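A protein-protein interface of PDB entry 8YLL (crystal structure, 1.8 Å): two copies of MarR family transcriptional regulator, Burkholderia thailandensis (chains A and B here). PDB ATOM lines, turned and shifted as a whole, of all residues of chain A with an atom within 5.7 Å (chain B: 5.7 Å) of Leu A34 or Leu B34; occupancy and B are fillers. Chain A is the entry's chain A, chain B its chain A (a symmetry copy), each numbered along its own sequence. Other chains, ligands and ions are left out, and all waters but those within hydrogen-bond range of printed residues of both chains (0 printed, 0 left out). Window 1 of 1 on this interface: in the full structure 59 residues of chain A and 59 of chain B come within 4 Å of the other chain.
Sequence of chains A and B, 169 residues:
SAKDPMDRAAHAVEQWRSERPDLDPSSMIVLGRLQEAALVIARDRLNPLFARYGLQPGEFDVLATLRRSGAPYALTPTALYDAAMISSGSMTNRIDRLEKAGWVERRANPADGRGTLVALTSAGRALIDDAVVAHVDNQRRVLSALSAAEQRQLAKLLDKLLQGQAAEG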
ATOM      1  N   ILE A  29      25.597 -16.904 -28.914  1.00  0.00           N
ATOM      2  CA  ILE A  29      24.669 -15.808 -29.176  1.00  0.00           C
ATOM      3  C   ILE A  29      24.372 -15.039 -27.893  1.00  0.00           C
ATOM      4  O   ILE A  29      24.596 -13.827 -27.816  1.00  0.00           O
ATOM      5  CB  ILE A  29      23.390 -16.323 -29.852  1.00  0.00           C
ATOM      6  CG1 ILE A  29      23.704 -16.690 -31.298  1.00  0.00           C
ATOM      7  CG2 ILE A  29      22.293 -15.264 -29.808  1.00  0.00           C
ATOM      8  CD1 ILE A  29      22.532 -17.206 -32.071  1.00  0.00           C
ATOM      9  N   VAL A  30      23.886 -15.729 -26.861  1.00  0.00           N
ATOM     10  CA  VAL A  30      23.497 -15.027 -25.636  1.00  0.00           C
ATOM     11  C   VAL A  30      24.704 -14.341 -24.991  1.00  0.00           C
ATOM     12  O   VAL A  30      24.612 -13.189 -24.544  1.00  0.00           O
ATOM     13  CB  VAL A  30      22.783 -15.992 -24.666  1.00  0.00           C
ATOM     14  CG1 VAL A  30      23.690 -17.097 -24.263  1.00  0.00           C
ATOM     15  CG2 VAL A  30      22.287 -15.254 -23.442  1.00  0.00           C
ATOM     16  N   LEU A  31      25.860 -15.010 -24.963  1.00  0.00           N
ATOM     17  CA  LEU A  31      27.015 -14.415 -24.293  1.00  0.00           C
ATOM     18  C   LEU A  31      27.652 -13.321 -25.140  1.00  0.00           C
ATOM     19  O   LEU A  31      28.152 -12.323 -24.601  1.00  0.00           O
ATOM     20  CB  LEU A  31      28.051 -15.492 -23.949  1.00  0.00           C
ATOM     21  CG  LEU A  31      27.621 -16.377 -22.770  1.00  0.00           C
ATOM     22  CD1 LEU A  31      28.607 -17.511 -22.521  1.00  0.00           C
ATOM     23  CD2 LEU A  31      27.460 -15.549 -21.508  1.00  0.00           C
ATOM     24  N   GLY A  32      27.668 -13.505 -26.458  1.00  0.00           N
ATOM     25  CA  GLY A  32      28.150 -12.445 -27.329  1.00  0.00           C
ATOM     26  C   GLY A  32      27.280 -11.204 -27.257  1.00  0.00           C
ATOM     27  O   GLY A  32      27.788 -10.077 -27.188  1.00  0.00           O
ATOM     28  N   ARG A  33      25.958 -11.392 -27.226  1.00  0.00           N
ATOM     29  CA  ARG A  33      25.071 -10.239 -27.110  1.00  0.00           C
ATOM     30  C   ARG A  33      25.167  -9.592 -25.741  1.00  0.00           C
ATOM     31  O   ARG A  33      25.050  -8.364 -25.631  1.00  0.00           O
ATOM     32  CB  ARG A  33      23.630 -10.645 -27.394  1.00  0.00           C
ATOM     33  CG  ARG A  33      23.352 -10.747 -28.872  1.00  0.00           C
ATOM     34  CD  ARG A  33      21.949 -11.177 -29.151  1.00  0.00           C
ATOM     35  NE  ARG A  33      21.832 -11.527 -30.552  1.00  0.00           N
ATOM     36  CZ  ARG A  33      20.856 -12.265 -31.058  1.00  0.00           C
ATOM     37  NH1 ARG A  33      19.886 -12.730 -30.275  1.00  0.00           N
ATOM     38  NH2 ARG A  33      20.854 -12.538 -32.347  1.00  0.00           N
ATOM     39  N   LEU A  34      25.366 -10.394 -24.699  1.00  0.00           N
ATOM     40  CA  LEU A  34      25.528  -9.854 -23.351  1.00  0.00           C
ATOM     41  C   LEU A  34      26.731  -8.921 -23.270  1.00  0.00           C
ATOM     42  O   LEU A  34      26.643  -7.803 -22.741  1.00  0.00           O
ATOM     43  CB  LEU A  34      25.667 -10.997 -22.348  1.00  0.00           C
ATOM     44  CG  LEU A  34      25.967 -10.546 -20.917  1.00  0.00           C
ATOM     45  CD1 LEU A  34      24.712  -9.998 -20.277  1.00  0.00           C
ATOM     46  CD2 LEU A  34      26.528 -11.672 -20.071  1.00  0.00           C
ATOM     47  N   GLN A  35      27.875  -9.377 -23.774  1.00  0.00           N
ATOM     48  CA  GLN A  35      29.095  -8.577 -23.693  1.00  0.00           C
ATOM     49  C   GLN A  35      29.028  -7.367 -24.625  1.00  0.00           C
ATOM     50  O   GLN A  35      29.506  -6.284 -24.279  1.00  0.00           O
ATOM     51  CB  GLN A  35      30.307  -9.445 -24.019  1.00  0.00           C
ATOM     52  CG  GLN A  35      30.548 -10.553 -22.980  1.00  0.00           C
ATOM     53  CD  GLN A  35      31.662 -11.504 -23.371  1.00  0.00           C
ATOM     54  OE1 GLN A  35      32.838 -11.170 -23.265  1.00  0.00           O
ATOM     55  NE2 GLN A  35      31.292 -12.698 -23.832  1.00  0.00           N
ATOM     56  N   GLU A  36      28.460  -7.530 -25.815  1.00  0.00           N
ATOM     57  CA  GLU A  36      28.365  -6.381 -26.719  1.00  0.00           C
ATOM     58  C   GLU A  36      27.402  -5.328 -26.191  1.00  0.00           C
ATOM     59  O   GLU A  36      27.635  -4.122 -26.379  1.00  0.00           O
ATOM     60  CB  GLU A  36      27.940  -6.829 -28.116  1.00  0.00           C
ATOM     61  CG  GLU A  36      27.811  -5.680 -29.149  1.00  0.00           C
ATOM     62  CD  GLU A  36      29.163  -5.153 -29.599  1.00  0.00           C
ATOM     63  OE1 GLU A  36      30.194  -5.590 -29.029  1.00  0.00           O
ATOM     64  OE2 GLU A  36      29.208  -4.315 -30.527  1.00  0.00           O
ATOM     65  N   ALA A  37      26.305  -5.755 -25.560  1.00  0.00           N
ATOM     66  CA  ALA A  37      25.360  -4.784 -25.021  1.00  0.00           C
ATOM     67  C   ALA A  37      25.988  -4.003 -23.877  1.00  0.00           C
ATOM     68  O   ALA A  37      25.860  -2.773 -23.817  1.00  0.00           O
ATOM     69  CB  ALA A  37      24.075  -5.478 -24.569  1.00  0.00           C
ATOM     70  N   ALA A  38      26.686  -4.697 -22.966  1.00  0.00           N
ATOM     71  CA  ALA A  38      27.364  -4.003 -21.875  1.00  0.00           C
ATOM     72  C   ALA A  38      28.383  -3.006 -22.415  1.00  0.00           C
ATOM     73  O   ALA A  38      28.492  -1.883 -21.912  1.00  0.00           O
ATOM     74  CB  ALA A  38      28.048  -5.007 -20.935  1.00  0.00           C
ATOM     75  N   LEU A  39      29.129  -3.399 -23.449  1.00  0.00           N
ATOM     76  CA  LEU A  39      30.192  -2.552 -23.975  1.00  0.00           C
ATOM     77  C   LEU A  39      29.615  -1.332 -24.697  1.00  0.00           C
ATOM     78  O   LEU A  39      30.022  -0.189 -24.443  1.00  0.00           O
ATOM     79  CB  LEU A  39      31.073  -3.372 -24.921  1.00  0.00           C
ATOM     80  CG  LEU A  39      32.103  -2.573 -25.723  1.00  0.00           C
ATOM     81  CD1 LEU A  39      32.995  -1.784 -24.795  1.00  0.00           C
ATOM     82  CD2 LEU A  39      32.935  -3.453 -26.650  1.00  0.00           C
ATOM     83  N   ILE A  41      26.679   0.053 -24.487  1.00  0.00           N
ATOM     84  CA  ILE A  41      25.939   0.949 -23.602  1.00  0.00           C
ATOM     85  C   ILE A  41      26.897   1.773 -22.751  1.00  0.00           C
ATOM     86  O   ILE A  41      26.723   2.992 -22.614  1.00  0.00           O
ATOM     87  CB  ILE A  41      24.932   0.149 -22.754  1.00  0.00           C
ATOM     88  CG1 ILE A  41      23.776  -0.328 -23.634  1.00  0.00           C
ATOM     89  CG2 ILE A  41      24.420   0.958 -21.573  1.00  0.00           C
ATOM     90  CD1 ILE A  41      22.880  -1.340 -22.945  1.00  0.00           C
ATOM     91  N   LEU A 158      18.922 -11.940 -15.886  1.00  0.00           N
ATOM     92  CA  LEU A 158      20.288 -11.558 -15.550  1.00  0.00           C
ATOM     93  C   LEU A 158      20.614 -11.911 -14.102  1.00  0.00           C
ATOM     94  O   LEU A 158      21.741 -12.326 -13.801  1.00  0.00           O
ATOM     95  CB  LEU A 158      20.507 -10.068 -15.821  1.00  0.00           C
ATOM     96  CG  LEU A 158      20.612  -9.677 -17.299  1.00  0.00           C
ATOM     97  CD1 LEU A 158      20.610  -8.167 -17.437  1.00  0.00           C
ATOM     98  CD2 LEU A 158      21.845 -10.274 -17.967  1.00  0.00           C
ATOM     99  N   LEU A 161      21.371 -15.685 -14.058  1.00  0.00           N
ATOM    100  CA  LEU A 161      22.699 -15.914 -14.626  1.00  0.00           C
ATOM    101  C   LEU A 161      23.799 -15.537 -13.638  1.00  0.00           C
ATOM    102  O   LEU A 161      24.773 -16.282 -13.456  1.00  0.00           O
ATOM    103  CB  LEU A 161      22.850 -15.116 -15.925  1.00  0.00           C
ATOM    104  CG  LEU A 161      24.117 -15.330 -16.760  1.00  0.00           C
ATOM    105  CD1 LEU A 161      24.201 -16.767 -17.239  1.00  0.00           C
ATOM    106  CD2 LEU A 161      24.149 -14.364 -17.942  1.00  0.00           C
ATOM    107  N   ILE B  29      18.516  -1.459 -11.875  1.00  0.00           N
ATOM    108  CA  ILE B  29      18.622  -2.897 -11.645  1.00  0.00           C
ATOM    109  C   ILE B  29      19.041  -3.614 -12.922  1.00  0.00           C
ATOM    110  O   ILE B  29      20.062  -4.309 -12.952  1.00  0.00           O
ATOM    111  CB  ILE B  29      17.313  -3.457 -11.069  1.00  0.00           C
ATOM    112  CG1 ILE B  29      17.177  -3.015  -9.616  1.00  0.00           C
ATOM    113  CG2 ILE B  29      17.293  -4.979 -11.156  1.00  0.00           C
ATOM    114  CD1 ILE B  29      15.937  -3.502  -8.936  1.00  0.00           C
ATOM    115  N   VAL B  30      18.280  -3.443 -14.003  1.00  0.00           N
ATOM    116  CA  VAL B  30      18.585  -4.179 -15.231  1.00  0.00           C
ATOM    117  C   VAL B  30      19.962  -3.791 -15.776  1.00  0.00           C
ATOM    118  O   VAL B  30      20.742  -4.657 -16.196  1.00  0.00           O
ATOM    119  CB  VAL B  30      17.464  -3.977 -16.272  1.00  0.00           C
ATOM    120  CG1 VAL B  30      17.347  -2.543 -16.645  1.00  0.00           C
ATOM    121  CG2 VAL B  30      17.719  -4.815 -17.507  1.00  0.00           C
ATOM    122  N   LEU B  31      20.303  -2.501 -15.745  1.00  0.00           N
ATOM    123  CA  LEU B  31      21.581  -2.085 -16.320  1.00  0.00           C
ATOM    124  C   LEU B  31      22.747  -2.429 -15.403  1.00  0.00           C
ATOM    125  O   LEU B  31      23.841  -2.765 -15.880  1.00  0.00           O
ATOM    126  CB  LEU B  31      21.569  -0.582 -16.625  1.00  0.00           C
ATOM    127  CG  LEU B  31      20.719  -0.229 -17.853  1.00  0.00           C
ATOM    128  CD1 LEU B  31      20.627   1.277 -18.067  1.00  0.00           C
ATOM    129  CD2 LEU B  31      21.277  -0.894 -19.100  1.00  0.00           C
ATOM    130  N   GLY B  32      22.541  -2.325 -14.093  1.00  0.00           N
ATOM    131  CA  GLY B  32      23.572  -2.755 -13.162  1.00  0.00           C
ATOM    132  C   GLY B  32      23.843  -4.246 -13.258  1.00  0.00           C
ATOM    133  O   GLY B  32      25.002  -4.680 -13.263  1.00  0.00           O
ATOM    134  N   ARG B  33      22.782  -5.047 -13.381  1.00  0.00           N
ATOM    135  CA  ARG B  33      22.982  -6.486 -13.525  1.00  0.00           C
ATOM    136  C   ARG B  33      23.599  -6.837 -14.866  1.00  0.00           C
ATOM    137  O   ARG B  33      24.393  -7.783 -14.949  1.00  0.00           O
ATOM    138  CB  ARG B  33      21.663  -7.227 -13.348  1.00  0.00           C
ATOM    139  CG  ARG B  33      21.297  -7.393 -11.895  1.00  0.00           C
ATOM    140  CD  ARG B  33      19.987  -8.091 -11.722  1.00  0.00           C
ATOM    141  NE  ARG B  33      19.564  -7.964 -10.342  1.00  0.00           N
ATOM    142  CZ  ARG B  33      18.322  -8.148  -9.923  1.00  0.00           C
ATOM    143  NH1 ARG B  33      17.363  -8.485 -10.780  1.00  0.00           N
ATOM    144  NH2 ARG B  33      18.042  -7.992  -8.643  1.00  0.00           N
ATOM    145  N   LEU B  34      23.240  -6.102 -15.915  1.00  0.00           N
ATOM    146  CA  LEU B  34      23.825  -6.332 -17.233  1.00  0.00           C
ATOM    147  C   LEU B  34      25.337  -6.135 -17.207  1.00  0.00           C
ATOM    148  O   LEU B  34      26.102  -6.973 -17.711  1.00  0.00           O
ATOM    149  CB  LEU B  34      23.182  -5.398 -18.256  1.00  0.00           C
ATOM    150  CG  LEU B  34      23.807  -5.464 -19.651  1.00  0.00           C
ATOM    151  CD1 LEU B  34      23.354  -6.722 -20.356  1.00  0.00           C
ATOM    152  CD2 LEU B  34      23.460  -4.249 -20.489  1.00  0.00           C
ATOM    153  N   GLN B  35      25.786  -5.018 -16.643  1.00  0.00           N
ATOM    154  CA  GLN B  35      27.216  -4.717 -16.620  1.00  0.00           C
ATOM    155  C   GLN B  35      27.963  -5.644 -15.661  1.00  0.00           C
ATOM    156  O   GLN B  35      29.089  -6.061 -15.945  1.00  0.00           O
ATOM    157  CB  GLN B  35      27.433  -3.255 -16.239  1.00  0.00           C
ATOM    158  CG  GLN B  35      26.887  -2.274 -17.289  1.00  0.00           C
ATOM    159  CD  GLN B  35      26.970  -0.825 -16.852  1.00  0.00           C
ATOM    160  OE1 GLN B  35      28.042  -0.225 -16.871  1.00  0.00           O
ATOM    161  NE2 GLN B  35      25.835  -0.256 -16.449  1.00  0.00           N
ATOM    162  N   GLU B  36      27.369  -5.964 -14.517  1.00  0.00           N
ATOM    163  CA  GLU B  36      28.056  -6.867 -13.590  1.00  0.00           C
ATOM    164  C   GLU B  36      28.158  -8.277 -14.151  1.00  0.00           C
ATOM    165  O   GLU B  36      29.165  -8.969 -13.915  1.00  0.00           O
ATOM    166  CB  GLU B  36      27.347  -6.891 -12.238  1.00  0.00           C
ATOM    167  CG  GLU B  36      28.001  -7.822 -11.184  1.00  0.00           C
ATOM    168  CD  GLU B  36      29.295  -7.249 -10.630  1.00  0.00           C
ATOM    169  OE1 GLU B  36      29.749  -6.195 -11.143  1.00  0.00           O
ATOM    170  OE2 GLU B  36      29.858  -7.834  -9.679  1.00  0.00           O
ATOM    171  N   ALA B  37      27.128  -8.735 -14.866  1.00  0.00           N
ATOM    172  CA  ALA B  37      27.185 -10.075 -15.439  1.00  0.00           C
ATOM    173  C   ALA B  37      28.257 -10.149 -16.516  1.00  0.00           C
ATOM    174  O   ALA B  37      29.040 -11.107 -16.550  1.00  0.00           O
ATOM    175  CB  ALA B  37      25.819 -10.482 -15.994  1.00  0.00           C
ATOM    176  N   ALA B  38      28.316  -9.141 -17.399  1.00  0.00           N
ATOM    177  CA  ALA B  38      29.356  -9.121 -18.421  1.00  0.00           C
ATOM    178  C   ALA B  38      30.743  -9.118 -17.788  1.00  0.00           C
ATOM    179  O   ALA B  38      31.647  -9.820 -18.252  1.00  0.00           O
ATOM    180  CB  ALA B  38      29.188  -7.902 -19.342  1.00  0.00           C
ATOM    181  N   LEU B  39      30.922  -8.341 -16.718  1.00  0.00           N
ATOM    182  CA  LEU B  39      32.233  -8.202 -16.101  1.00  0.00           C
ATOM    183  C   LEU B  39      32.642  -9.490 -15.384  1.00  0.00           C
ATOM    184  O   LEU B  39      33.754 -10.003 -15.580  1.00  0.00           O
ATOM    185  CB  LEU B  39      32.210  -7.024 -15.121  1.00  0.00           C
ATOM    186  CG  LEU B  39      33.447  -6.882 -14.231  1.00  0.00           C
ATOM    187  CD1 LEU B  39      34.694  -6.782 -15.076  1.00  0.00           C
ATOM    188  CD2 LEU B  39      33.347  -5.697 -13.274  1.00  0.00           C
ATOM    189  N   ILE B  41      31.571 -12.541 -15.751  1.00  0.00           N
ATOM    190  CA  ILE B  41      31.744 -13.672 -16.657  1.00  0.00           C
ATOM    191  C   ILE B  41      33.058 -13.552 -17.420  1.00  0.00           C
ATOM    192  O   ILE B  41      33.806 -14.533 -17.535  1.00  0.00           O
ATOM    193  CB  ILE B  41      30.526 -13.797 -17.592  1.00  0.00           C
ATOM    194  CG1 ILE B  41      29.317 -14.303 -16.804  1.00  0.00           C
ATOM    195  CG2 ILE B  41      30.817 -14.698 -18.782  1.00  0.00           C
ATOM    196  CD1 ILE B  41      28.016 -14.205 -17.580  1.00  0.00           C
ATOM    197  N   LEU B 158      18.198  -9.327 -25.173  1.00  0.00           N
ATOM    198  CA  LEU B 158      19.452  -8.622 -25.410  1.00  0.00           C
ATOM    199  C   LEU B 158      19.527  -8.102 -26.840  1.00  0.00           C
ATOM    200  O   LEU B 158      20.046  -7.003 -27.078  1.00  0.00           O
ATOM    201  CB  LEU B 158      20.642  -9.526 -25.083  1.00  0.00           C
ATOM    202  CG  LEU B 158      20.894  -9.769 -23.590  1.00  0.00           C
ATOM    203  CD1 LEU B 158      21.953 -10.840 -23.411  1.00  0.00           C
ATOM    204  CD2 LEU B 158      21.296  -8.493 -22.859  1.00  0.00           C
ATOM    205  N   LEU B 161      17.391  -4.901 -26.939  1.00  0.00           N
ATOM    206  CA  LEU B 161      18.125  -3.815 -26.289  1.00  0.00           C
ATOM    207  C   LEU B 161      19.231  -3.275 -27.193  1.00  0.00           C
ATOM    208  O   LEU B 161      19.401  -2.055 -27.329  1.00  0.00           O
ATOM    209  CB  LEU B 161      18.710  -4.307 -24.962  1.00  0.00           C
ATOM    210  CG  LEU B 161      19.395  -3.282 -24.051  1.00  0.00           C
ATOM    211  CD1 LEU B 161      18.405  -2.222 -23.608  1.00  0.00           C
ATOM    212  CD2 LEU B 161      20.023  -3.973 -22.844  1.00  0.00           C
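Among the printed residues, pairs that only touch across the chains: Val A30 with Leu B158 (3.7 Å), Arg A33 with Leu B158 (3.9 Å), Leu A34 with Leu B34 (3.5 Å), Leu A34 with Ile B41 (3.9 Å), Leu A34 with Leu B158 (3.7 Å), Ala A38 with Ala B38 (3.5 Å), Ile A41 with Leu B34 (3.9 Å), Ile A41 with Leu B161 (3.9 Å), Leu A158 with Val B30 (3.7 Å), Leu A158 with Arg B33 (3.9 Å), Leu A158 with Leu B34 (3.7 Å) and Leu A161 with Ile B41 (3.9 Å).
Of the printed residues of chain B, Val A30 touches Leu B158 (3.7 Å).
Printed residues of chain B within 4 Å of Leu A34: Leu B34, Ile B41 and Leu B158.
Glu A36 touches none of the printed residues of chain B.
Of the printed residues of chain B, Ile A41 touches Leu B34 and Leu B161.
Of the printed residues of chain A, Arg B33 touches Leu A158.
Leu B34 touches just these residues of chain A: Leu A34, Ile A41 and Leu A158.
Leu B39 touches none of the printed residues of chain A.
Of the printed residues of chain A, Ile B41 touches Leu A34 and Leu A161.
The nearest residue of chain A that does not touch Leu B34 is Ala A38 (4.1 Å).
Of the 14 printed residues of chain B, 7 touch a printed residue of chain A.
Printed residues of chain B that touch a printed residue of chain A: Val B30, Arg B33, Leu B34, Ala B38, Ile B41, Leu B158 and Leu B161.
Hydrophobic or aromatic side chains of chain A within 4 Å of the printed part of chain B: Leu A34, Ala A38, Ile A41, Leu A158 and Leu A161.
Leu A34 touches its own counterpart, Leu B34.
Leu A34 touches Ile B41, and with the chains exchanged Ile A41 touches Leu B34.
Leu A34 touches Leu B158, and with the chains exchanged Leu A158 touches Leu B34.
Ile A41 touches Leu B161, and with the chains exchanged Leu A161 touches Ile B41.
14 positions are printed for both chains.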
